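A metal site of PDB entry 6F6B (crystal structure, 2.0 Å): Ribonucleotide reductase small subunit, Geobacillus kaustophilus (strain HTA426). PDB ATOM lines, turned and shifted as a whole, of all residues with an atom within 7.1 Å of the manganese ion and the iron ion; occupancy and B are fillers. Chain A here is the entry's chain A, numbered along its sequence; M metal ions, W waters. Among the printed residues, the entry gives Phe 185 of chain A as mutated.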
ATOM      1  N   GLY A  82      37.080 -25.828  -7.018  1.00  0.00           N
ATOM      2  CA  GLY A  82      35.715 -26.102  -7.446  1.00  0.00           C
ATOM      3  C   GLY A  82      35.115 -24.948  -8.244  1.00  0.00           C
ATOM      4  O   GLY A  82      34.610 -25.154  -9.347  1.00  0.00           O
ATOM      5  N   GLU A  83      35.237 -23.732  -7.717  1.00  0.00           N
ATOM      6  CA  GLU A  83      34.734 -22.533  -8.377  1.00  0.00           C
ATOM      7  C   GLU A  83      35.478 -22.250  -9.691  1.00  0.00           C
ATOM      8  O   GLU A  83      34.870 -21.919 -10.710  1.00  0.00           O
ATOM      9  CB  GLU A  83      34.856 -21.322  -7.445  1.00  0.00           C
ATOM     10  CG  GLU A  83      34.034 -21.496  -6.135  1.00  0.00           C
ATOM     11  CD  GLU A  83      32.510 -21.696  -6.339  1.00  0.00           C
ATOM     12  OE1 GLU A  83      31.984 -21.451  -7.429  1.00  0.00           O
ATOM     13  OE2 GLU A  83      31.831 -22.107  -5.358  1.00  0.00           O
ATOM     14  N   VAL A  86      34.241 -24.728 -12.407  1.00  0.00           N
ATOM     15  CA  VAL A  86      32.889 -24.547 -12.968  1.00  0.00           C
ATOM     16  C   VAL A  86      32.809 -23.246 -13.736  1.00  0.00           C
ATOM     17  O   VAL A  86      31.945 -23.067 -14.639  1.00  0.00           O
ATOM     18  CB  VAL A  86      31.765 -24.560 -11.857  1.00  0.00           C
ATOM     19  CG1 VAL A  86      31.721 -25.900 -11.167  1.00  0.00           C
ATOM     20  CG2 VAL A  86      32.001 -23.453 -10.848  1.00  0.00           C
ATOM     21  N   THR A  87      33.692 -22.309 -13.390  1.00  0.00           N
ATOM     22  CA  THR A  87      33.821 -21.082 -14.181  1.00  0.00           C
ATOM     23  C   THR A  87      34.193 -21.482 -15.604  1.00  0.00           C
ATOM     24  O   THR A  87      33.561 -21.057 -16.600  1.00  0.00           O
ATOM     25  CB  THR A  87      34.875 -20.106 -13.608  1.00  0.00           C
ATOM     26  OG1 THR A  87      34.492 -19.649 -12.303  1.00  0.00           O
ATOM     27  CG2 THR A  87      35.073 -18.903 -14.530  1.00  0.00           C
ATOM     28  N   PHE A 112      25.234 -16.719 -15.225  1.00  0.00           N
ATOM     29  CA  PHE A 112      25.725 -17.925 -14.530  1.00  0.00           C
ATOM     30  C   PHE A 112      27.261 -17.870 -14.472  1.00  0.00           C
ATOM     31  O   PHE A 112      27.896 -18.083 -13.448  1.00  0.00           O
ATOM     32  CB  PHE A 112      25.195 -19.164 -15.304  1.00  0.00           C
ATOM     33  CG  PHE A 112      25.403 -20.484 -14.645  1.00  0.00           C
ATOM     34  CD1 PHE A 112      24.312 -21.308 -14.405  1.00  0.00           C
ATOM     35  CD2 PHE A 112      26.654 -20.941 -14.291  1.00  0.00           C
ATOM     36  CE1 PHE A 112      24.473 -22.575 -13.829  1.00  0.00           C
ATOM     37  CE2 PHE A 112      26.812 -22.180 -13.702  1.00  0.00           C
ATOM     38  CZ  PHE A 112      25.712 -23.002 -13.485  1.00  0.00           C
ATOM     39  N   ASP A 115      28.631 -14.979 -12.376  1.00  0.00           N
ATOM     40  CA  ASP A 115      28.563 -15.408 -10.973  1.00  0.00           C
ATOM     41  C   ASP A 115      29.764 -16.288 -10.605  1.00  0.00           C
ATOM     42  O   ASP A 115      30.361 -16.120  -9.542  1.00  0.00           O
ATOM     43  CB  ASP A 115      27.305 -16.215 -10.657  1.00  0.00           C
ATOM     44  CG  ASP A 115      26.032 -15.445 -10.774  1.00  0.00           C
ATOM     45  OD1 ASP A 115      26.023 -14.207 -10.669  1.00  0.00           O
ATOM     46  OD2 ASP A 115      25.000 -16.114 -10.939  1.00  0.00           O
ATOM     47  N   GLU A 116      30.072 -17.278 -11.443  1.00  0.00           N
ATOM     48  CA  GLU A 116      31.131 -18.205 -11.072  1.00  0.00           C
ATOM     49  C   GLU A 116      32.475 -17.441 -11.011  1.00  0.00           C
ATOM     50  O   GLU A 116      33.323 -17.653 -10.110  1.00  0.00           O
ATOM     51  CB  GLU A 116      31.255 -19.379 -12.057  1.00  0.00           C
ATOM     52  CG  GLU A 116      30.043 -20.297 -12.246  1.00  0.00           C
ATOM     53  CD  GLU A 116      29.459 -20.906 -10.960  1.00  0.00           C
ATOM     54  OE1 GLU A 116      29.995 -20.738  -9.878  1.00  0.00           O
ATOM     55  OE2 GLU A 116      28.492 -21.671 -11.081  1.00  0.00           O
ATOM     56  N   ALA A 117      32.669 -16.535 -11.961  1.00  0.00           N
ATOM     57  CA  ALA A 117      33.869 -15.707 -11.961  1.00  0.00           C
ATOM     58  C   ALA A 117      34.045 -15.008 -10.624  1.00  0.00           C
ATOM     59  O   ALA A 117      35.095 -15.074 -10.035  1.00  0.00           O
ATOM     60  CB  ALA A 117      33.811 -14.720 -13.077  1.00  0.00           C
ATOM     61  N   LYS A 118      32.976 -14.392 -10.131  1.00  0.00           N
ATOM     62  CA  LYS A 118      33.000 -13.807  -8.829  1.00  0.00           C
ATOM     63  C   LYS A 118      33.242 -14.831  -7.728  1.00  0.00           C
ATOM     64  O   LYS A 118      33.801 -14.449  -6.722  1.00  0.00           O
ATOM     65  CB  LYS A 118      31.697 -13.061  -8.500  1.00  0.00           C
ATOM     66  CG  LYS A 118      31.317 -12.001  -9.566  1.00  0.00           C
ATOM     67  CD  LYS A 118      30.273 -10.989  -9.053  1.00  0.00           C
ATOM     68  CE  LYS A 118      28.904 -11.577  -8.849  1.00  0.00           C
ATOM     69  NZ  LYS A 118      27.824 -10.533  -8.791  1.00  0.00           N
ATOM     70  N   HIS A 119      32.822 -16.091  -7.882  1.00  0.00           N
ATOM     71  CA  HIS A 119      33.052 -17.068  -6.825  1.00  0.00           C
ATOM     72  C   HIS A 119      34.497 -17.446  -6.711  1.00  0.00           C
ATOM     73  O   HIS A 119      35.029 -17.486  -5.599  1.00  0.00           O
ATOM     74  CB  HIS A 119      32.217 -18.347  -7.011  1.00  0.00           C
ATOM     75  CG  HIS A 119      30.756 -18.072  -7.013  1.00  0.00           C
ATOM     76  ND1 HIS A 119      29.823 -18.983  -7.461  1.00  0.00           N
ATOM     77  CD2 HIS A 119      30.076 -16.963  -6.648  1.00  0.00           C
ATOM     78  CE1 HIS A 119      28.630 -18.433  -7.366  1.00  0.00           C
ATOM     79  NE2 HIS A 119      28.760 -17.202  -6.885  1.00  0.00           N
ATOM     80  N   VAL A 120      35.130 -17.692  -7.852  1.00  0.00           N
ATOM     81  CA  VAL A 120      36.582 -17.892  -7.891  1.00  0.00           C
ATOM     82  C   VAL A 120      37.321 -16.699  -7.318  1.00  0.00           C
ATOM     83  O   VAL A 120      38.307 -16.863  -6.599  1.00  0.00           O
ATOM     84  CB  VAL A 120      37.159 -18.069  -9.298  1.00  0.00           C
ATOM     85  CG1 VAL A 120      38.605 -18.539  -9.189  1.00  0.00           C
ATOM     86  CG2 VAL A 120      36.444 -19.086 -10.031  1.00  0.00           C
ATOM     87  N   PHE A 123      37.048 -16.553  -3.193  1.00  0.00           N
ATOM     88  CA  PHE A 123      37.976 -17.394  -2.489  1.00  0.00           C
ATOM     89  C   PHE A 123      39.426 -16.980  -2.677  1.00  0.00           C
ATOM     90  O   PHE A 123      40.214 -17.086  -1.750  1.00  0.00           O
ATOM     91  CB  PHE A 123      37.811 -18.830  -2.911  1.00  0.00           C
ATOM     92  CG  PHE A 123      36.566 -19.480  -2.321  1.00  0.00           C
ATOM     93  CD1 PHE A 123      36.498 -19.764  -0.974  1.00  0.00           C
ATOM     94  CD2 PHE A 123      35.456 -19.769  -3.106  1.00  0.00           C
ATOM     95  CE1 PHE A 123      35.359 -20.355  -0.402  1.00  0.00           C
ATOM     96  CE2 PHE A 123      34.299 -20.372  -2.546  1.00  0.00           C
ATOM     97  CZ  PHE A 123      34.272 -20.661  -1.188  1.00  0.00           C
ATOM     98  N   TYR A 176      27.349 -31.389 -13.469  1.00  0.00           N
ATOM     99  CA  TYR A 176      27.675 -29.990 -13.136  1.00  0.00           C
ATOM    100  C   TYR A 176      26.694 -29.470 -12.044  1.00  0.00           C
ATOM    101  O   TYR A 176      27.074 -29.098 -10.951  1.00  0.00           O
ATOM    102  CB  TYR A 176      27.588 -29.121 -14.384  1.00  0.00           C
ATOM    103  CG  TYR A 176      28.113 -27.710 -14.226  1.00  0.00           C
ATOM    104  CD1 TYR A 176      29.179 -27.278 -15.000  1.00  0.00           C
ATOM    105  CD2 TYR A 176      27.544 -26.810 -13.360  1.00  0.00           C
ATOM    106  CE1 TYR A 176      29.679 -25.990 -14.887  1.00  0.00           C
ATOM    107  CE2 TYR A 176      28.025 -25.497 -13.269  1.00  0.00           C
ATOM    108  CZ  TYR A 176      29.096 -25.095 -14.039  1.00  0.00           C
ATOM    109  OH  TYR A 176      29.608 -23.801 -13.944  1.00  0.00           O
ATOM    110  N   ASN A 177      25.436 -29.432 -12.396  1.00  0.00           N
ATOM    111  CA  ASN A 177      24.456 -28.779 -11.569  1.00  0.00           C
ATOM    112  C   ASN A 177      23.926 -29.609 -10.418  1.00  0.00           C
ATOM    113  O   ASN A 177      23.748 -29.081  -9.338  1.00  0.00           O
ATOM    114  CB  ASN A 177      23.274 -28.321 -12.417  1.00  0.00           C
ATOM    115  CG  ASN A 177      23.701 -27.539 -13.624  1.00  0.00           C
ATOM    116  OD1 ASN A 177      23.746 -28.042 -14.716  1.00  0.00           O
ATOM    117  ND2 ASN A 177      24.032 -26.284 -13.426  1.00  0.00           N
ATOM    118  N   GLU A 181      27.479 -28.832  -7.984  1.00  0.00           N
ATOM    119  CA  GLU A 181      26.869 -27.681  -7.347  1.00  0.00           C
ATOM    120  C   GLU A 181      25.777 -28.133  -6.371  1.00  0.00           C
ATOM    121  O   GLU A 181      25.760 -27.677  -5.259  1.00  0.00           O
ATOM    122  CB  GLU A 181      26.305 -26.692  -8.369  1.00  0.00           C
ATOM    123  CG  GLU A 181      27.426 -26.108  -9.340  1.00  0.00           C
ATOM    124  CD  GLU A 181      27.303 -24.651  -9.653  1.00  0.00           C
ATOM    125  OE1 GLU A 181      26.484 -24.308 -10.531  1.00  0.00           O
ATOM    126  OE2 GLU A 181      28.086 -23.834  -9.072  1.00  0.00           O
ATOM    127  N   PHE A 185      28.860 -28.713  -3.429  1.00  0.00           N
ATOM    128  CA  PHE A 185      28.973 -27.335  -2.997  1.00  0.00           C
ATOM    129  C   PHE A 185      27.897 -27.009  -1.935  1.00  0.00           C
ATOM    130  O   PHE A 185      28.224 -26.333  -0.946  1.00  0.00           O
ATOM    131  CB  PHE A 185      28.864 -26.374  -4.170  1.00  0.00           C
ATOM    132  CG  PHE A 185      30.084 -26.367  -5.116  1.00  0.00           C
ATOM    133  CD1 PHE A 185      31.266 -26.986  -4.786  1.00  0.00           C
ATOM    134  CD2 PHE A 185      30.006 -25.716  -6.317  1.00  0.00           C
ATOM    135  CE1 PHE A 185      32.365 -26.946  -5.668  1.00  0.00           C
ATOM    136  CE2 PHE A 185      31.100 -25.681  -7.211  1.00  0.00           C
ATOM    137  CZ  PHE A 185      32.248 -26.275  -6.879  1.00  0.00           C
ATOM    138  N   TYR A 189      28.828 -25.530   1.753  1.00  0.00           N
ATOM    139  CA  TYR A 189      28.433 -24.236   2.297  1.00  0.00           C
ATOM    140  C   TYR A 189      27.816 -24.439   3.674  1.00  0.00           C
ATOM    141  O   TYR A 189      28.003 -23.619   4.560  1.00  0.00           O
ATOM    142  CB  TYR A 189      27.357 -23.521   1.458  1.00  0.00           C
ATOM    143  CG  TYR A 189      27.591 -23.381  -0.012  1.00  0.00           C
ATOM    144  CD1 TYR A 189      28.870 -23.208  -0.547  1.00  0.00           C
ATOM    145  CD2 TYR A 189      26.483 -23.387  -0.881  1.00  0.00           C
ATOM    146  CE1 TYR A 189      29.038 -23.086  -1.900  1.00  0.00           C
ATOM    147  CE2 TYR A 189      26.635 -23.264  -2.228  1.00  0.00           C
ATOM    148  CZ  TYR A 189      27.915 -23.113  -2.752  1.00  0.00           C
ATOM    149  OH  TYR A 189      28.075 -22.990  -4.111  1.00  0.00           O
ATOM    150  N   LEU A 212      27.264 -16.095  -2.371  1.00  0.00           N
ATOM    151  CA  LEU A 212      27.477 -17.207  -3.258  1.00  0.00           C
ATOM    152  C   LEU A 212      26.307 -18.161  -3.224  1.00  0.00           C
ATOM    153  O   LEU A 212      25.801 -18.613  -4.254  1.00  0.00           O
ATOM    154  CB  LEU A 212      28.766 -17.879  -2.847  1.00  0.00           C
ATOM    155  CG  LEU A 212      29.384 -18.981  -3.633  1.00  0.00           C
ATOM    156  CD1 LEU A 212      30.906 -18.959  -3.432  1.00  0.00           C
ATOM    157  CD2 LEU A 212      28.817 -20.234  -3.098  1.00  0.00           C
ATOM    158  N   ASP A 215      23.487 -16.850  -5.288  1.00  0.00           N
ATOM    159  CA  ASP A 215      23.659 -17.032  -6.721  1.00  0.00           C
ATOM    160  C   ASP A 215      23.335 -18.472  -7.084  1.00  0.00           C
ATOM    161  O   ASP A 215      22.739 -18.748  -8.119  1.00  0.00           O
ATOM    162  CB  ASP A 215      25.098 -16.711  -7.190  1.00  0.00           C
ATOM    163  CG  ASP A 215      25.500 -15.295  -6.952  1.00  0.00           C
ATOM    164  OD1 ASP A 215      24.651 -14.382  -6.984  1.00  0.00           O
ATOM    165  OD2 ASP A 215      26.712 -15.105  -6.772  1.00  0.00           O
ATOM    166  N   GLU A 216      23.803 -19.403  -6.270  1.00  0.00           N
ATOM    167  CA  GLU A 216      23.761 -20.820  -6.672  1.00  0.00           C
ATOM    168  C   GLU A 216      22.341 -21.384  -6.696  1.00  0.00           C
ATOM    169  O   GLU A 216      22.067 -22.285  -7.433  1.00  0.00           O
ATOM    170  CB  GLU A 216      24.671 -21.632  -5.769  1.00  0.00           C
ATOM    171  CG  GLU A 216      26.161 -21.330  -5.969  1.00  0.00           C
ATOM    172  CD  GLU A 216      26.651 -21.733  -7.332  1.00  0.00           C
ATOM    173  OE1 GLU A 216      26.024 -22.644  -7.843  1.00  0.00           O
ATOM    174  OE2 GLU A 216      27.638 -21.145  -7.893  1.00  0.00           O
ATOM    175  N   GLY A 217      21.435 -20.780  -5.920  1.00  0.00           N
ATOM    176  CA  GLY A 217      20.010 -21.030  -6.084  1.00  0.00           C
ATOM    177  C   GLY A 217      19.504 -20.899  -7.529  1.00  0.00           C
ATOM    178  O   GLY A 217      18.728 -21.750  -8.019  1.00  0.00           O
ATOM    179  N   ARG A 218      19.923 -19.848  -8.236  1.00  0.00           N
ATOM    180  CA  ARG A 218      19.585 -19.767  -9.654  1.00  0.00           C
ATOM    181  C   ARG A 218      20.221 -20.842 -10.479  1.00  0.00           C
ATOM    182  O   ARG A 218      19.598 -21.377 -11.404  1.00  0.00           O
ATOM    183  CB  ARG A 218      19.942 -18.420 -10.268  1.00  0.00           C
ATOM    184  CG  ARG A 218      19.228 -17.258  -9.581  1.00  0.00           C
ATOM    185  CD  ARG A 218      19.481 -15.958 -10.286  1.00  0.00           C
ATOM    186  NE  ARG A 218      20.912 -15.581 -10.249  1.00  0.00           N
ATOM    187  CZ  ARG A 218      21.536 -14.936  -9.243  1.00  0.00           C
ATOM    188  NH1 ARG A 218      20.896 -14.551  -8.170  1.00  0.00           N
ATOM    189  NH2 ARG A 218      22.833 -14.665  -9.339  1.00  0.00           N
ATOM    190  N   HIS A 219      21.478 -21.132 -10.204  1.00  0.00           N
ATOM    191  CA  HIS A 219      22.205 -22.097 -11.032  1.00  0.00           C
ATOM    192  C   HIS A 219      21.530 -23.475 -11.044  1.00  0.00           C
ATOM    193  O   HIS A 219      21.456 -24.151 -12.089  1.00  0.00           O
ATOM    194  CB  HIS A 219      23.655 -22.257 -10.560  1.00  0.00           C
ATOM    195  CG  HIS A 219      24.457 -20.998 -10.623  1.00  0.00           C
ATOM    196  ND1 HIS A 219      25.829 -20.969 -10.468  1.00  0.00           N
ATOM    197  CD2 HIS A 219      24.068 -19.708 -10.790  1.00  0.00           C
ATOM    198  CE1 HIS A 219      26.241 -19.713 -10.505  1.00  0.00           C
ATOM    199  NE2 HIS A 219      25.200 -18.932 -10.716  1.00  0.00           N
ATOM    200  N   ILE A 220      21.089 -23.917  -9.883  1.00  0.00           N
ATOM    201  CA  ILE A 220      20.453 -25.241  -9.778  1.00  0.00           C
ATOM    202  C   ILE A 220      19.090 -25.238 -10.475  1.00  0.00           C
ATOM    203  O   ILE A 220      18.675 -26.251 -11.039  1.00  0.00           O
ATOM    204  CB  ILE A 220      20.331 -25.645  -8.302  1.00  0.00           C
ATOM    205  CG1 ILE A 220      19.724 -27.033  -8.126  1.00  0.00           C
ATOM    206  CG2 ILE A 220      19.491 -24.639  -7.606  1.00  0.00           C
ATOM    207  CD1 ILE A 220      20.629 -28.078  -8.618  1.00  0.00           C
HETATM  208 MN    MN M   1      29.897 -21.037  -7.824  1.00  0.00          MN
HETATM  209 FE    FE M   2      27.072 -22.356  -9.769  1.00  0.00          FE
HETATM  210  O   HOH W   1      29.141 -22.616  -6.542  1.00  0.00           O
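O of Asp 115 sits close to NE2 of His 119 (3.3 Å). A ring nitrogen (NE2) of His 219 sits at hydrogen-bond distance from the side-chain carboxylate (OD2) of Asp 115 (2.8 Å). The backbone carbonyl oxygen of Glu 83 sits at hydrogen-bond distance from the side-chain hydroxyl of Thr 87, at 2.8 Å. The side-chain hydroxyl of Thr 87 lies within hydrogen-bond range of the backbone carbonyl oxygen of Glu 116 (3.2 Å). A ring nitrogen (NE2) of His 119 lies within hydrogen-bond range of the side-chain carboxylate (OD2) of Asp 215. The backbone carbonyl oxygen of Tyr 176 is in hydrogen-bond range of the backbone NH of Glu 181.
Five residues have an atom within 4 Å of the manganese ion: Glu 83, Glu 116, His 119, Glu 181 and Glu 216. The nearest printed residue that does not touch the manganese ion is Val 86 (4.4 Å).
Phe 112 touches the iron ion (CE2 to FE, 3.9 Å). Within 4 Å of the iron ion: Phe 112, Glu 116, Glu 181, Glu 216 and His 219.
The manganese ion is bound by OE1 of Glu 116 (2.1 Å), ND1 of His 119 (2.1 Å), OE1 of Glu 83 (2.2 Å), water W1 (2.2 Å) and OE2 of Glu 216 (2.3 Å). The manganese ion has five donor atoms within binding distance.
The iron ion is bound by the side-chain carboxylate (OE2) of Glu 181 (1.9 Å), a ring nitrogen (ND1) of His 219 (2.0 Å), the side-chain carboxylate (OE2) of Glu 116 (2.1 Å), the side-chain carboxylate (OE1) of Glu 181 (2.2 Å), the side-chain carboxylate (OE1) of Glu 216 (2.2 Å) and the side-chain carboxylate (OE2) of Glu 216 (2.3 Å).
Water W1 lies within hydrogen-bond range of OH of Tyr 189 (2.7 Å) and OE2 of Glu 83 (3.0 Å).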
